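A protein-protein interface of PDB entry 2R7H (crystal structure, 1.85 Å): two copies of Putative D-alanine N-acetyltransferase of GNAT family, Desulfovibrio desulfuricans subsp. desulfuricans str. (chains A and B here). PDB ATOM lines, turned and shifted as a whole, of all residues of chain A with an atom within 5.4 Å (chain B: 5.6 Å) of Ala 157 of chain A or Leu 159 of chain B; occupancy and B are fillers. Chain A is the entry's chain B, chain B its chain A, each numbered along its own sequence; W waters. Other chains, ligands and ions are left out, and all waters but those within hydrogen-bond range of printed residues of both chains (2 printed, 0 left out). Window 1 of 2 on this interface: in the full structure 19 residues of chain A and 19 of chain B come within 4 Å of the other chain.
Printed residues of chain B within 4 Å of Phe 132 of chain A: Phe 162 (3.7 Å). Of the printed residues of chain B, Glu 156 of chain A touches Val 158 (3.6 Å), Leu 159 (3.6 Å) and Lys 160 (3.0 Å). Ala 157 of chain A touches just these residues of chain B: Ala 157 and Leu 159. Ile 170 of chain A touches none of the printed residues of chain B. Ile 171 of chain A touches none of the printed residues of chain B. Printed residues of chain B within 4 Å of Arg 173 of chain A: Lys 160. Printed residues of chain A within 4 Å of Ala 157 of chain B: Ala 157 (3.3 Å) and Leu 159 (3.7 Å). Leu 159 of chain B touches just these residues of chain A: Glu 156 (3.6 Å) and Ala 157 (3.8 Å). The nearest printed residue of chain B that does not touch Phe 132 of chain A is Leu 159 of chain B (4.3 Å).
Of the 11 printed residues of chain B, 5 touch a printed residue of chain A. Printed residues of chain B that touch a printed residue of chain A: Ala 157, Val 158, Leu 159, Lys 160 and Phe 162. Hydrophobic or aromatic side chains of chain B within 4 Å of the printed part of chain A: Ala 157, Leu 159 and Phe 162. Among the printed residues, 8 pairs touch across the chains. Among the printed residues, no Asp or Glu carboxylate lies within 4 Å of a Lys or Arg side-chain nitrogen of the other chain.
N of Lys 160 of chain B sits at hydrogen-bond distance from OE2 of Glu 156 of chain A, at 3.0 Å. The guanidinium group of Arg 173 of chain A is in hydrogen-bond range of the backbone carbonyl oxygen of Lys 160 of chain B, at 2.9 Å.
Ala 157 of chain B touches its own counterpart, Ala 157 of chain A. Ala 157 of chain A touches Leu 159 of chain B, and with the chains exchanged Leu 159 of chain A touches Ala 157 of chain B. Positions printed for both chains: 157, 158, 159, 169, 170 and 171. Of the 8 pairs that touch across the chains among the printed residues, 3 have their exchanged pair printed and touching as well.
CE2 of Phe 132 of chain A touches CD2 of Phe 162 of chain B, 3.7 Å away. Val 158 of chain B touches Glu 156 of chain A (O to OE2, 3.6 Å). Leu 159 of chain B touches Glu 156 of chain A. Ala 157 of chain A touches Ala 157 of chain B. Leu 159 of chain B touches Ala 157 of chain A. Ala 157 of chain B touches Leu 159 of chain A (CB to CD2, 3.7 Å).
The backbone NH of Ile 171 of chain B is in hydrogen-bond range of the backbone carbonyl oxygen of Ala 157 of chain B. N of Leu 159 of chain B lies within hydrogen-bond range of O of Lys 169 of chain B (2.9 Å). The side-chain amino group (NZ) of Lys 160 of chain B is in salt-bridge range of the side-chain carboxylate (OD2) of Asp 168 of chain B (3.1 Å). N of Phe 162 of chain B is in hydrogen-bond range of O of Asp 167 of chain B (3.1 Å). N of Glu 156 of chain A is in hydrogen-bond range of O of Ile 171 of chain A, at 2.7 Å. OE1 of Glu 156 of chain A lies within salt-bridge range of NH1 of Arg 173 of chain A (2.9 Å).
Water W2 bridges O of Val 158 of chain B (2.6 Å) and OE2 of Glu 156 of chain A (2.7 Å). Water W1 bridges the backbone carbonyl oxygen (O) of Glu 156 of chain A (2.7 Å) and the backbone NH (N) of Val 158 of chain B (3.2 Å).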
ATOM      1  N   PHE A 132      -6.219   5.253  13.719  1.00  0.00           N
ATOM      2  CA  PHE A 132      -6.290   5.886  15.005  1.00  0.00           C
ATOM      3  C   PHE A 132      -6.131   7.400  14.894  1.00  0.00           C
ATOM      4  O   PHE A 132      -5.416   7.867  14.052  1.00  0.00           O
ATOM      5  CB  PHE A 132      -5.218   5.344  15.964  1.00  0.00           C
ATOM      6  CG  PHE A 132      -5.494   3.963  16.449  1.00  0.00           C
ATOM      7  CD1 PHE A 132      -6.398   3.751  17.481  1.00  0.00           C
ATOM      8  CD2 PHE A 132      -4.909   2.867  15.850  1.00  0.00           C
ATOM      9  CE1 PHE A 132      -6.641   2.501  17.906  1.00  0.00           C
ATOM     10  CE2 PHE A 132      -5.171   1.637  16.248  1.00  0.00           C
ATOM     11  CZ  PHE A 132      -6.036   1.429  17.305  1.00  0.00           C
ATOM     12  N   ALA A 155     -14.046   6.178  21.155  1.00  0.00           N
ATOM     13  CA  ALA A 155     -13.069   6.575  22.136  1.00  0.00           C
ATOM     14  C   ALA A 155     -12.612   5.273  22.756  1.00  0.00           C
ATOM     15  O   ALA A 155     -13.381   4.638  23.445  1.00  0.00           O
ATOM     16  CB  ALA A 155     -13.752   7.459  23.203  1.00  0.00           C
ATOM     17  N   GLU A 156     -11.386   4.832  22.497  1.00  0.00           N
ATOM     18  CA  GLU A 156     -10.895   3.557  23.085  1.00  0.00           C
ATOM     19  C   GLU A 156      -9.985   3.696  24.308  1.00  0.00           C
ATOM     20  O   GLU A 156      -9.889   2.751  25.093  1.00  0.00           O
ATOM     21  CB  GLU A 156     -10.239   2.691  22.020  1.00  0.00           C
ATOM     22  CG  GLU A 156      -9.840   1.290  22.499  1.00  0.00           C
ATOM     23  CD  GLU A 156      -9.314   0.412  21.421  1.00  0.00           C
ATOM     24  OE1 GLU A 156      -8.745   0.946  20.450  1.00  0.00           O
ATOM     25  OE2 GLU A 156      -9.405  -0.831  21.582  1.00  0.00           O
ATOM     26  N   ALA A 157      -9.317   4.838  24.477  1.00  0.00           N
ATOM     27  CA  ALA A 157      -8.414   5.051  25.609  1.00  0.00           C
ATOM     28  C   ALA A 157      -8.376   6.523  25.984  1.00  0.00           C
ATOM     29  O   ALA A 157      -8.536   7.402  25.127  1.00  0.00           O
ATOM     30  CB  ALA A 157      -7.005   4.590  25.234  1.00  0.00           C
ATOM     31  N   VAL A 158      -8.123   6.755  27.271  1.00  0.00           N
ATOM     32  CA  VAL A 158      -7.999   8.060  27.884  1.00  0.00           C
ATOM     33  C   VAL A 158      -6.729   7.975  28.745  1.00  0.00           C
ATOM     34  O   VAL A 158      -6.587   7.049  29.527  1.00  0.00           O
ATOM     35  CB  VAL A 158      -9.249   8.389  28.747  1.00  0.00           C
ATOM     36  CG1 VAL A 158      -9.120   9.777  29.406  1.00  0.00           C
ATOM     37  CG2 VAL A 158     -10.511   8.333  27.908  1.00  0.00           C
ATOM     38  N   LEU A 159      -5.750   8.841  28.469  1.00  0.00           N
ATOM     39  CA  LEU A 159      -4.518   8.928  29.229  1.00  0.00           C
ATOM     40  C   LEU A 159      -4.674  10.252  29.991  1.00  0.00           C
ATOM     41  O   LEU A 159      -4.597  11.323  29.385  1.00  0.00           O
ATOM     42  CB  LEU A 159      -3.262   8.855  28.325  1.00  0.00           C
ATOM     43  CG  LEU A 159      -3.155   7.602  27.393  1.00  0.00           C
ATOM     44  CD1 LEU A 159      -1.792   7.646  26.685  1.00  0.00           C
ATOM     45  CD2 LEU A 159      -3.336   6.262  28.131  1.00  0.00           C
ATOM     46  N   LYS A 169      -5.382  12.937  26.919  1.00  0.00           N
ATOM     47  CA  LYS A 169      -5.287  12.526  25.525  1.00  0.00           C
ATOM     48  C   LYS A 169      -6.356  11.493  25.379  1.00  0.00           C
ATOM     49  O   LYS A 169      -6.396  10.580  26.205  1.00  0.00           O
ATOM     50  CB  LYS A 169      -3.936  11.883  25.162  1.00  0.00           C
ATOM     51  CG  LYS A 169      -3.868  11.518  23.631  1.00  0.00           C
ATOM     52  CD  LYS A 169      -2.489  11.225  23.142  1.00  0.00           C
ATOM     53  CE  LYS A 169      -1.934   9.973  23.613  1.00  0.00           C
ATOM     54  NZ  LYS A 169      -0.659   9.673  22.851  1.00  0.00           N
ATOM     55  N   ILE A 170      -7.213  11.631  24.356  1.00  0.00           N
ATOM     56  CA  ILE A 170      -8.272  10.655  24.071  1.00  0.00           C
ATOM     57  C   ILE A 170      -7.846   9.996  22.756  1.00  0.00           C
ATOM     58  O   ILE A 170      -7.499  10.704  21.798  1.00  0.00           O
ATOM     59  CB  ILE A 170      -9.701  11.236  23.912  1.00  0.00           C
ATOM     60  CG1 ILE A 170     -10.206  11.920  25.191  1.00  0.00           C
ATOM     61  CG2 ILE A 170     -10.707  10.072  23.597  1.00  0.00           C
ATOM     62  CD1 ILE A 170      -9.471  13.090  25.606  1.00  0.00           C
ATOM     63  N   ILE A 171      -7.855   8.663  22.724  1.00  0.00           N
ATOM     64  CA  ILE A 171      -7.454   7.901  21.528  1.00  0.00           C
ATOM     65  C   ILE A 171      -8.719   7.298  20.947  1.00  0.00           C
ATOM     66  O   ILE A 171      -9.452   6.552  21.634  1.00  0.00           O
ATOM     67  CB  ILE A 171      -6.401   6.805  21.807  1.00  0.00           C
ATOM     68  CG1 ILE A 171      -5.151   7.396  22.497  1.00  0.00           C
ATOM     69  CG2 ILE A 171      -5.985   6.148  20.481  1.00  0.00           C
ATOM     70  CD1 ILE A 171      -4.087   6.363  22.948  1.00  0.00           C
ATOM     71  N   ARG A 173     -10.569   5.210  17.836  1.00  0.00           N
ATOM     72  CA  ARG A 173     -10.322   4.070  16.972  1.00  0.00           C
ATOM     73  C   ARG A 173     -11.354   3.956  15.829  1.00  0.00           C
ATOM     74  O   ARG A 173     -12.537   4.078  16.079  1.00  0.00           O
ATOM     75  CB  ARG A 173     -10.526   2.830  17.851  1.00  0.00           C
ATOM     76  CG  ARG A 173     -10.313   1.461  17.199  1.00  0.00           C
ATOM     77  CD  ARG A 173     -11.024   0.448  18.011  1.00  0.00           C
ATOM     78  NE  ARG A 173     -10.810  -0.887  17.489  1.00  0.00           N
ATOM     79  CZ  ARG A 173      -9.733  -1.617  17.720  1.00  0.00           C
ATOM     80  NH1 ARG A 173      -8.696  -1.138  18.420  1.00  0.00           N
ATOM     81  NH2 ARG A 173      -9.677  -2.825  17.182  1.00  0.00           N
ATOM     82  N   ALA B 157      -4.531   2.026  29.451  1.00  0.00           N
ATOM     83  CA  ALA B 157      -5.260   1.849  28.194  1.00  0.00           C
ATOM     84  C   ALA B 157      -4.858   0.563  27.489  1.00  0.00           C
ATOM     85  O   ALA B 157      -3.756   0.098  27.655  1.00  0.00           O
ATOM     86  CB  ALA B 157      -4.916   3.017  27.256  1.00  0.00           C
ATOM     87  N   VAL B 158      -5.802  -0.023  26.751  1.00  0.00           N
ATOM     88  CA  VAL B 158      -5.588  -1.211  25.900  1.00  0.00           C
ATOM     89  C   VAL B 158      -6.168  -0.855  24.546  1.00  0.00           C
ATOM     90  O   VAL B 158      -7.311  -0.408  24.491  1.00  0.00           O
ATOM     91  CB  VAL B 158      -6.283  -2.477  26.354  1.00  0.00           C
ATOM     92  CG1 VAL B 158      -5.976  -3.626  25.330  1.00  0.00           C
ATOM     93  CG2 VAL B 158      -5.827  -2.847  27.724  1.00  0.00           C
ATOM     94  N   LEU B 159      -5.326  -0.828  23.498  1.00  0.00           N
ATOM     95  CA  LEU B 159      -5.771  -0.600  22.153  1.00  0.00           C
ATOM     96  C   LEU B 159      -5.769  -1.985  21.498  1.00  0.00           C
ATOM     97  O   LEU B 159      -4.724  -2.597  21.275  1.00  0.00           O
ATOM     98  CB  LEU B 159      -4.873   0.350  21.389  1.00  0.00           C
ATOM     99  CG  LEU B 159      -4.746   1.681  22.059  1.00  0.00           C
ATOM    100  CD1 LEU B 159      -3.749   2.403  21.096  1.00  0.00           C
ATOM    101  CD2 LEU B 159      -6.043   2.509  22.244  1.00  0.00           C
ATOM    102  N   LYS B 160      -6.969  -2.489  21.252  1.00  0.00           N
ATOM    103  CA  LYS B 160      -7.116  -3.841  20.724  1.00  0.00           C
ATOM    104  C   LYS B 160      -6.576  -4.069  19.317  1.00  0.00           C
ATOM    105  O   LYS B 160      -6.754  -3.263  18.423  1.00  0.00           O
ATOM    106  CB  LYS B 160      -8.577  -4.241  20.699  1.00  0.00           C
ATOM    107  CG  LYS B 160      -9.353  -4.187  22.067  1.00  0.00           C
ATOM    108  CD  LYS B 160      -8.901  -5.148  23.178  1.00  0.00           C
ATOM    109  CE  LYS B 160      -9.167  -6.576  22.763  1.00  0.00           C
ATOM    110  NZ  LYS B 160      -8.900  -7.528  23.838  1.00  0.00           N
ATOM    111  N   ALA B 161      -5.830  -5.156  19.164  1.00  0.00           N
ATOM    112  CA  ALA B 161      -5.303  -5.634  17.909  1.00  0.00           C
ATOM    113  C   ALA B 161      -4.502  -4.546  17.357  1.00  0.00           C
ATOM    114  O   ALA B 161      -4.437  -4.354  16.124  1.00  0.00           O
ATOM    115  CB  ALA B 161      -6.405  -6.008  16.928  1.00  0.00           C
ATOM    116  N   PHE B 162      -3.845  -3.809  18.241  1.00  0.00           N
ATOM    117  CA  PHE B 162      -2.996  -2.677  17.672  1.00  0.00           C
ATOM    118  C   PHE B 162      -1.787  -3.010  16.829  1.00  0.00           C
ATOM    119  O   PHE B 162      -1.532  -2.326  15.784  1.00  0.00           O
ATOM    120  CB  PHE B 162      -2.538  -1.823  18.878  1.00  0.00           C
ATOM    121  CG  PHE B 162      -1.701  -0.603  18.495  1.00  0.00           C
ATOM    122  CD1 PHE B 162      -0.328  -0.680  18.432  1.00  0.00           C
ATOM    123  CD2 PHE B 162      -2.314   0.593  18.284  1.00  0.00           C
ATOM    124  CE1 PHE B 162       0.424   0.432  18.058  1.00  0.00           C
ATOM    125  CE2 PHE B 162      -1.575   1.706  17.952  1.00  0.00           C
ATOM    126  CZ  PHE B 162      -0.218   1.610  17.825  1.00  0.00           C
ATOM    127  N   ASP B 167      -3.040  -8.864  18.464  1.00  0.00           N
ATOM    128  CA  ASP B 167      -1.885  -8.400  19.266  1.00  0.00           C
ATOM    129  C   ASP B 167      -2.192  -7.002  19.820  1.00  0.00           C
ATOM    130  O   ASP B 167      -1.913  -6.016  19.215  1.00  0.00           O
ATOM    131  CB  ASP B 167      -0.656  -8.391  18.347  1.00  0.00           C
ATOM    132  CG  ASP B 167       0.649  -8.267  19.075  1.00  0.00           C
ATOM    133  OD1 ASP B 167       0.704  -7.805  20.245  1.00  0.00           O
ATOM    134  OD2 ASP B 167       1.679  -8.577  18.434  1.00  0.00           O
ATOM    135  N   ASP B 168      -2.746  -6.934  21.009  1.00  0.00           N
ATOM    136  CA  ASP B 168      -3.112  -5.650  21.592  1.00  0.00           C
ATOM    137  C   ASP B 168      -1.949  -4.890  22.199  1.00  0.00           C
ATOM    138  O   ASP B 168      -1.012  -5.527  22.698  1.00  0.00           O
ATOM    139  CB  ASP B 168      -4.000  -5.932  22.784  1.00  0.00           C
ATOM    140  CG  ASP B 168      -5.213  -6.655  22.454  1.00  0.00           C
ATOM    141  OD1 ASP B 168      -5.582  -6.807  21.284  1.00  0.00           O
ATOM    142  OD2 ASP B 168      -5.818  -7.154  23.430  1.00  0.00           O
ATOM    143  N   LYS B 169      -2.036  -3.550  22.245  1.00  0.00           N
ATOM    144  CA  LYS B 169      -1.026  -2.710  22.884  1.00  0.00           C
ATOM    145  C   LYS B 169      -1.588  -2.291  24.244  1.00  0.00           C
ATOM    146  O   LYS B 169      -2.707  -1.833  24.308  1.00  0.00           O
ATOM    147  CB  LYS B 169      -0.709  -1.466  22.058  1.00  0.00           C
ATOM    148  CG  LYS B 169       0.356  -0.590  22.750  1.00  0.00           C
ATOM    149  CD  LYS B 169       0.871   0.489  21.909  1.00  0.00           C
ATOM    150  CE  LYS B 169      -0.061   1.570  21.577  1.00  0.00           C
ATOM    151  NZ  LYS B 169       0.798   2.647  20.884  1.00  0.00           N
ATOM    152  N   ILE B 170      -0.827  -2.483  25.327  1.00  0.00           N
ATOM    153  CA  ILE B 170      -1.222  -2.090  26.697  1.00  0.00           C
ATOM    154  C   ILE B 170      -0.336  -0.848  26.971  1.00  0.00           C
ATOM    155  O   ILE B 170       0.850  -0.935  26.744  1.00  0.00           O
ATOM    156  CB  ILE B 170      -0.950  -3.193  27.784  1.00  0.00           C
ATOM    157  CG1 ILE B 170      -1.681  -4.510  27.537  1.00  0.00           C
ATOM    158  CG2 ILE B 170      -1.565  -2.801  29.153  1.00  0.00           C
ATOM    159  CD1 ILE B 170      -1.321  -5.275  26.368  1.00  0.00           C
ATOM    160  N   ILE B 171      -0.923   0.274  27.398  1.00  0.00           N
ATOM    161  CA  ILE B 171      -0.193   1.514  27.689  1.00  0.00           C
ATOM    162  C   ILE B 171      -0.134   1.577  29.227  1.00  0.00           C
ATOM    163  O   ILE B 171      -1.188   1.543  29.929  1.00  0.00           O
ATOM    164  CB  ILE B 171      -0.784   2.787  27.085  1.00  0.00           C
ATOM    165  CG1 ILE B 171      -0.974   2.638  25.579  1.00  0.00           C
ATOM    166  CG2 ILE B 171       0.132   4.059  27.453  1.00  0.00           C
ATOM    167  CD1 ILE B 171      -1.519   3.861  24.883  1.00  0.00           C
HETATM  168  O   HOH W   1      -8.549   1.573  27.068  1.00  0.00           O
HETATM  169  O   HOH W   2      -9.603  -1.560  24.174  1.00  0.00           O
